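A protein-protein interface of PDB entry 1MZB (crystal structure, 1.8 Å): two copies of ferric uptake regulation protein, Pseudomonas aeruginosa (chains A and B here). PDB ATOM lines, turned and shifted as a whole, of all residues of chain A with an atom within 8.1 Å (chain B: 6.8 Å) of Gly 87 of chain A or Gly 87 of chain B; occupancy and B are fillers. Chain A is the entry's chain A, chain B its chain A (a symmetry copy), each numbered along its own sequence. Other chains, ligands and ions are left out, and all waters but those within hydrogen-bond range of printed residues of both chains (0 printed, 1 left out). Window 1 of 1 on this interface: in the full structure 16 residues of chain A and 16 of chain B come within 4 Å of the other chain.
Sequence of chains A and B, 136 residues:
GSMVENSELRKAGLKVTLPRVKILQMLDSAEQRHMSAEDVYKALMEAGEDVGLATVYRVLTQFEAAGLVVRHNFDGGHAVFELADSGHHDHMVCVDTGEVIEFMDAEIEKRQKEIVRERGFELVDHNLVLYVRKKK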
ATOM      1  N   GLU A  82      12.868   2.453  20.498  1.00  0.00           N
ATOM      2  CA  GLU A  82      12.781   1.336  21.442  1.00  0.00           C
ATOM      3  C   GLU A  82      14.069   1.294  22.229  1.00  0.00           C
ATOM      4  O   GLU A  82      15.078   1.788  21.780  1.00  0.00           O
ATOM      5  CB  GLU A  82      12.547   0.005  20.719  1.00  0.00           C
ATOM      6  CG  GLU A  82      13.585  -0.342  19.636  1.00  0.00           C
ATOM      7  CD  GLU A  82      13.178  -1.568  18.793  1.00  0.00           C
ATOM      8  OE1 GLU A  82      13.150  -2.693  19.322  1.00  0.00           O
ATOM      9  OE2 GLU A  82      12.886  -1.394  17.595  1.00  0.00           O
ATOM     10  N   LEU A  83      14.013   0.762  23.434  1.00  0.00           N
ATOM     11  CA  LEU A  83      15.214   0.685  24.229  1.00  0.00           C
ATOM     12  C   LEU A  83      16.292  -0.133  23.524  1.00  0.00           C
ATOM     13  O   LEU A  83      16.010  -1.029  22.703  1.00  0.00           O
ATOM     14  CB  LEU A  83      14.887   0.059  25.577  1.00  0.00           C
ATOM     15  CG  LEU A  83      13.936   0.902  26.409  1.00  0.00           C
ATOM     16  CD1 LEU A  83      13.519   0.084  27.635  1.00  0.00           C
ATOM     17  CD2 LEU A  83      14.628   2.238  26.829  1.00  0.00           C
ATOM     18  N   ALA A  84      17.536   0.200  23.845  1.00  0.00           N
ATOM     19  CA  ALA A  84      18.690  -0.480  23.294  1.00  0.00           C
ATOM     20  C   ALA A  84      19.080  -1.563  24.308  1.00  0.00           C
ATOM     21  O   ALA A  84      19.390  -2.688  23.924  1.00  0.00           O
ATOM     22  CB  ALA A  84      19.849   0.522  23.093  1.00  0.00           C
ATOM     23  N   ASP A  85      19.009  -1.214  25.600  1.00  0.00           N
ATOM     24  CA  ASP A  85      19.367  -2.116  26.710  1.00  0.00           C
ATOM     25  C   ASP A  85      18.747  -3.517  26.667  1.00  0.00           C
ATOM     26  O   ASP A  85      19.379  -4.492  27.098  1.00  0.00           O
ATOM     27  CB  ASP A  85      19.060  -1.456  28.080  1.00  0.00           C
ATOM     28  CG  ASP A  85      17.606  -0.998  28.216  1.00  0.00           C
ATOM     29  OD1 ASP A  85      17.140  -0.218  27.357  1.00  0.00           O
ATOM     30  OD2 ASP A  85      16.922  -1.402  29.183  1.00  0.00           O
ATOM     31  N   SER A  86      17.524  -3.619  26.146  1.00  0.00           N
ATOM     32  CA  SER A  86      16.820  -4.895  26.055  1.00  0.00           C
ATOM     33  C   SER A  86      17.635  -5.920  25.265  1.00  0.00           C
ATOM     34  O   SER A  86      18.557  -5.553  24.524  1.00  0.00           O
ATOM     35  CB  SER A  86      15.458  -4.692  25.375  1.00  0.00           C
ATOM     36  OG  SER A  86      15.624  -4.223  24.044  1.00  0.00           O
ATOM     37  N   GLY A  87      17.297  -7.199  25.419  1.00  0.00           N
ATOM     38  CA  GLY A  87      18.012  -8.221  24.675  1.00  0.00           C
ATOM     39  C   GLY A  87      17.995  -7.812  23.210  1.00  0.00           C
ATOM     40  O   GLY A  87      17.087  -7.091  22.779  1.00  0.00           O
ATOM     41  N   HIS A  88      18.991  -8.243  22.446  1.00  0.00           N
ATOM     42  CA  HIS A  88      19.050  -7.890  21.026  1.00  0.00           C
ATOM     43  C   HIS A  88      17.913  -8.532  20.247  1.00  0.00           C
ATOM     44  O   HIS A  88      17.468  -9.650  20.557  1.00  0.00           O
ATOM     45  CB  HIS A  88      20.386  -8.326  20.415  1.00  0.00           C
ATOM     46  CG  HIS A  88      20.424  -8.271  18.912  1.00  0.00           C
ATOM     47  ND1 HIS A  88      20.467  -7.085  18.206  1.00  0.00           N
ATOM     48  CD2 HIS A  88      20.487  -9.262  17.988  1.00  0.00           C
ATOM     49  CE1 HIS A  88      20.565  -7.353  16.914  1.00  0.00           C
ATOM     50  NE2 HIS A  88      20.583  -8.670  16.752  1.00  0.00           N
ATOM     51  N   HIS A  89      17.459  -7.814  19.227  1.00  0.00           N
ATOM     52  CA  HIS A  89      16.385  -8.283  18.373  1.00  0.00           C
ATOM     53  C   HIS A  89      16.473  -7.596  17.014  1.00  0.00           C
ATOM     54  O   HIS A  89      16.776  -6.410  16.910  1.00  0.00           O
ATOM     55  CB  HIS A  89      15.026  -7.993  19.029  1.00  0.00           C
ATOM     56  N   ASP A  90      16.262  -8.369  15.963  1.00  0.00           N
ATOM     57  CA  ASP A  90      16.248  -7.809  14.620  1.00  0.00           C
ATOM     58  C   ASP A  90      14.757  -7.840  14.330  1.00  0.00           C
ATOM     59  O   ASP A  90      13.998  -8.194  15.209  1.00  0.00           O
ATOM     60  CB  ASP A  90      17.029  -8.690  13.707  1.00  0.00           C
ATOM     61  CG  ASP A  90      18.495  -8.779  14.145  1.00  0.00           C
ATOM     62  OD1 ASP A  90      19.117  -7.733  14.357  1.00  0.00           O
ATOM     63  OD2 ASP A  90      18.970  -9.862  14.261  1.00  0.00           O
ATOM     64  N   GLU A 102       9.644  -9.125  16.187  1.00  0.00           N
ATOM     65  CA  GLU A 102      11.049  -9.240  16.576  1.00  0.00           C
ATOM     66  C   GLU A 102      11.520 -10.700  16.500  1.00  0.00           C
ATOM     67  O   GLU A 102      10.743 -11.644  16.709  1.00  0.00           O
ATOM     68  CB  GLU A 102      11.273  -8.749  18.013  1.00  0.00           C
ATOM     69  CG  GLU A 102      11.174  -7.244  18.198  1.00  0.00           C
ATOM     70  CD  GLU A 102      11.657  -6.787  19.571  1.00  0.00           C
ATOM     71  OE1 GLU A 102      11.611  -7.604  20.521  1.00  0.00           O
ATOM     72  OE2 GLU A 102      12.062  -5.611  19.708  1.00  0.00           O
ATOM     73  N   PHE A 103      12.799 -10.885  16.192  1.00  0.00           N
ATOM     74  CA  PHE A 103      13.384 -12.222  16.171  1.00  0.00           C
ATOM     75  C   PHE A 103      14.856 -12.077  16.471  1.00  0.00           C
ATOM     76  O   PHE A 103      15.411 -10.981  16.405  1.00  0.00           O
ATOM     77  CB  PHE A 103      13.178 -12.931  14.833  1.00  0.00           C
ATOM     78  CG  PHE A 103      14.021 -12.398  13.705  1.00  0.00           C
ATOM     79  CD1 PHE A 103      13.594 -11.301  12.942  1.00  0.00           C
ATOM     80  CD2 PHE A 103      15.229 -12.996  13.402  1.00  0.00           C
ATOM     81  CE1 PHE A 103      14.373 -10.817  11.878  1.00  0.00           C
ATOM     82  CE2 PHE A 103      16.033 -12.522  12.346  1.00  0.00           C
ATOM     83  CZ  PHE A 103      15.598 -11.432  11.582  1.00  0.00           C
ATOM     84  N   MET A 104      15.484 -13.179  16.836  1.00  0.00           N
ATOM     85  CA  MET A 104      16.905 -13.191  17.131  1.00  0.00           C
ATOM     86  C   MET A 104      17.356 -14.588  16.735  1.00  0.00           C
ATOM     87  O   MET A 104      16.930 -15.586  17.334  1.00  0.00           O
ATOM     88  CB  MET A 104      17.133 -12.971  18.622  1.00  0.00           C
ATOM     89  CG  MET A 104      18.363 -13.677  19.167  1.00  0.00           C
ATOM     90  SD  MET A 104      19.849 -12.756  18.911  1.00  0.00           S
ATOM     91  CE  MET A 104      19.777 -11.654  20.329  1.00  0.00           C
ATOM     92  N   ASP A 105      18.175 -14.669  15.702  1.00  0.00           N
ATOM     93  CA  ASP A 105      18.638 -15.964  15.243  1.00  0.00           C
ATOM     94  C   ASP A 105      20.129 -16.099  15.551  1.00  0.00           C
ATOM     95  O   ASP A 105      20.941 -15.413  14.941  1.00  0.00           O
ATOM     96  CB  ASP A 105      18.437 -16.096  13.745  1.00  0.00           C
ATOM     97  CG  ASP A 105      18.736 -17.495  13.271  1.00  0.00           C
ATOM     98  OD1 ASP A 105      18.099 -18.420  13.803  1.00  0.00           O
ATOM     99  OD2 ASP A 105      19.602 -17.679  12.410  1.00  0.00           O
ATOM    100  N   ALA A 106      20.487 -17.005  16.460  1.00  0.00           N
ATOM    101  CA  ALA A 106      21.894 -17.163  16.825  1.00  0.00           C
ATOM    102  C   ALA A 106      22.768 -17.551  15.618  1.00  0.00           C
ATOM    103  O   ALA A 106      23.924 -17.168  15.554  1.00  0.00           O
ATOM    104  CB  ALA A 106      22.032 -18.216  17.956  1.00  0.00           C
ATOM    105  N   GLU A 109      23.559 -14.319  13.778  1.00  0.00           N
ATOM    106  CA  GLU A 109      24.445 -13.492  14.597  1.00  0.00           C
ATOM    107  C   GLU A 109      25.890 -14.002  14.559  1.00  0.00           C
ATOM    108  O   GLU A 109      26.840 -13.216  14.493  1.00  0.00           O
ATOM    109  CB  GLU A 109      23.963 -13.470  16.055  1.00  0.00           C
ATOM    110  CG  GLU A 109      22.562 -12.888  16.285  1.00  0.00           C
ATOM    111  CD  GLU A 109      22.413 -11.460  15.782  1.00  0.00           C
ATOM    112  OE1 GLU A 109      23.325 -10.638  16.000  1.00  0.00           O
ATOM    113  OE2 GLU A 109      21.356 -11.165  15.189  1.00  0.00           O
ATOM    114  N   LEU B  83      21.005 -21.621  24.188  1.00  0.00           N
ATOM    115  CA  LEU B  83      22.167 -20.775  24.306  1.00  0.00           C
ATOM    116  C   LEU B  83      21.948 -19.678  25.343  1.00  0.00           C
ATOM    117  O   LEU B  83      20.811 -19.243  25.616  1.00  0.00           O
ATOM    118  CB  LEU B  83      22.479 -20.155  22.952  1.00  0.00           C
ATOM    119  CG  LEU B  83      22.864 -21.182  21.902  1.00  0.00           C
ATOM    120  CD1 LEU B  83      22.947 -20.472  20.547  1.00  0.00           C
ATOM    121  CD2 LEU B  83      24.225 -21.849  22.275  1.00  0.00           C
ATOM    122  N   ALA B  84      23.057 -19.245  25.932  1.00  0.00           N
ATOM    123  CA  ALA B  84      23.050 -18.193  26.926  1.00  0.00           C
ATOM    124  C   ALA B  84      23.344 -16.887  26.177  1.00  0.00           C
ATOM    125  O   ALA B  84      22.708 -15.867  26.434  1.00  0.00           O
ATOM    126  CB  ALA B  84      24.134 -18.464  27.993  1.00  0.00           C
ATOM    127  N   ASP B  85      24.278 -16.955  25.218  1.00  0.00           N
ATOM    128  CA  ASP B  85      24.707 -15.796  24.412  1.00  0.00           C
ATOM    129  C   ASP B  85      23.586 -14.962  23.782  1.00  0.00           C
ATOM    130  O   ASP B  85      23.721 -13.738  23.647  1.00  0.00           O
ATOM    131  CB  ASP B  85      25.710 -16.231  23.311  1.00  0.00           C
ATOM    132  CG  ASP B  85      25.169 -17.337  22.404  1.00  0.00           C
ATOM    133  OD1 ASP B  85      24.768 -18.400  22.928  1.00  0.00           O
ATOM    134  OD2 ASP B  85      25.149 -17.162  21.165  1.00  0.00           O
ATOM    135  N   SER B  86      22.487 -15.616  23.406  1.00  0.00           N
ATOM    136  CA  SER B  86      21.351 -14.938  22.785  1.00  0.00           C
ATOM    137  C   SER B  86      20.817 -13.822  23.685  1.00  0.00           C
ATOM    138  O   SER B  86      21.099 -13.797  24.890  1.00  0.00           O
ATOM    139  CB  SER B  86      20.230 -15.950  22.505  1.00  0.00           C
ATOM    140  OG  SER B  86      19.751 -16.520  23.716  1.00  0.00           O
ATOM    141  N   GLY B  87      20.048 -12.903  23.103  1.00  0.00           N
ATOM    142  CA  GLY B  87      19.484 -11.832  23.904  1.00  0.00           C
ATOM    143  C   GLY B  87      18.785 -12.474  25.093  1.00  0.00           C
ATOM    144  O   GLY B  87      18.354 -13.631  25.007  1.00  0.00           O
ATOM    145  N   HIS B  88      18.681 -11.753  26.202  1.00  0.00           N
ATOM    146  CA  HIS B  88      18.025 -12.300  27.391  1.00  0.00           C
ATOM    147  C   HIS B  88      16.539 -12.512  27.156  1.00  0.00           C
ATOM    148  O   HIS B  88      15.885 -11.751  26.422  1.00  0.00           O
ATOM    149  CB  HIS B  88      18.215 -11.367  28.592  1.00  0.00           C
ATOM    150  CG  HIS B  88      17.342 -11.695  29.771  1.00  0.00           C
ATOM    151  ND1 HIS B  88      17.547 -12.800  30.573  1.00  0.00           N
ATOM    152  CD2 HIS B  88      16.296 -11.023  30.317  1.00  0.00           C
ATOM    153  CE1 HIS B  88      16.670 -12.784  31.565  1.00  0.00           C
ATOM    154  NE2 HIS B  88      15.899 -11.713  31.436  1.00  0.00           N
ATOM    155  N   HIS B  89      16.013 -13.548  27.797  1.00  0.00           N
ATOM    156  CA  HIS B  89      14.607 -13.887  27.694  1.00  0.00           C
ATOM    157  C   HIS B  89      14.178 -14.684  28.921  1.00  0.00           C
ATOM    158  O   HIS B  89      14.909 -15.534  29.425  1.00  0.00           O
ATOM    159  CB  HIS B  89      14.355 -14.701  26.415  1.00  0.00           C
ATOM    160  N   GLU B 102       8.824 -17.120  25.039  1.00  0.00           N
ATOM    161  CA  GLU B 102       9.838 -16.217  25.586  1.00  0.00           C
ATOM    162  C   GLU B 102       9.313 -14.775  25.641  1.00  0.00           C
ATOM    163  O   GLU B 102       8.492 -14.351  24.814  1.00  0.00           O
ATOM    164  CB  GLU B 102      11.110 -16.222  24.726  1.00  0.00           C
ATOM    165  CG  GLU B 102      11.946 -17.486  24.826  1.00  0.00           C
ATOM    166  CD  GLU B 102      13.314 -17.341  24.169  1.00  0.00           C
ATOM    167  OE1 GLU B 102      13.448 -16.496  23.253  1.00  0.00           O
ATOM    168  OE2 GLU B 102      14.249 -18.082  24.549  1.00  0.00           O
ATOM    169  N   MET B 104      10.587 -10.591  27.328  1.00  0.00           N
ATOM    170  CA  MET B 104      11.606  -9.786  27.977  1.00  0.00           C
ATOM    171  C   MET B 104      10.905  -8.470  28.276  1.00  0.00           C
ATOM    172  O   MET B 104      10.503  -7.741  27.357  1.00  0.00           O
ATOM    173  CB  MET B 104      12.773  -9.552  27.025  1.00  0.00           C
ATOM    174  CG  MET B 104      13.472  -8.218  27.225  1.00  0.00           C
ATOM    175  SD  MET B 104      14.675  -8.265  28.520  1.00  0.00           S
ATOM    176  CE  MET B 104      16.076  -8.934  27.616  1.00  0.00           C
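Gly 87 of chain A touches its own counterpart, Gly 87 of chain B. Gly 87 of chain A touches His 88 of chain B, and with the chains exchanged His 88 of chain A touches Gly 87 of chain B. Gly 87 of chain A touches Met 104 of chain B, and with the chains exchanged Met 104 of chain A touches Gly 87 of chain B.
OG of Ser 86 of chain B lies within hydrogen-bond range of O of Leu 83 of chain B.
Of chain B, only Gly 87 (3.97 Å), His 88 (3.9 Å) and Met 104 (3.1 Å) come within 4 Å of Gly 87 of chain A. Of the printed residues of chain B, Met 104 of chain A touches Gly 87. No residue of chain A comes within 4 Å of Ser 86 of chain B. Gly 87 of chain B touches just these residues of chain A: Gly 87, His 88 and Met 104. Of the printed residues of chain A, His 88 of chain B touches Gly 87. The nearest residue of chain A that does not touch Gly 87 of chain B is Ser 86 of chain A (6.3 Å). The nearest printed residue of chain B that does not touch His 88 of chain A is His 88 of chain B (5.2 Å).
Among the printed residues, pairs that only touch across the chains: Gly 87 of chain A with Met 104 of chain B, Met 104 of chain A with Gly 87 of chain B, Ala 106 of chain A with Leu 83 of chain B, His 88 of chain A with Gly 87 of chain B, Gly 87 of chain A with His 88 of chain B and Gly 87 of chain A with Gly 87 of chain B.
Printed residues of chain A that touch a printed residue of chain B: Gly 87, His 88, Met 104 and Ala 106. Among the printed residues, 6 pairs touch across the chains.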
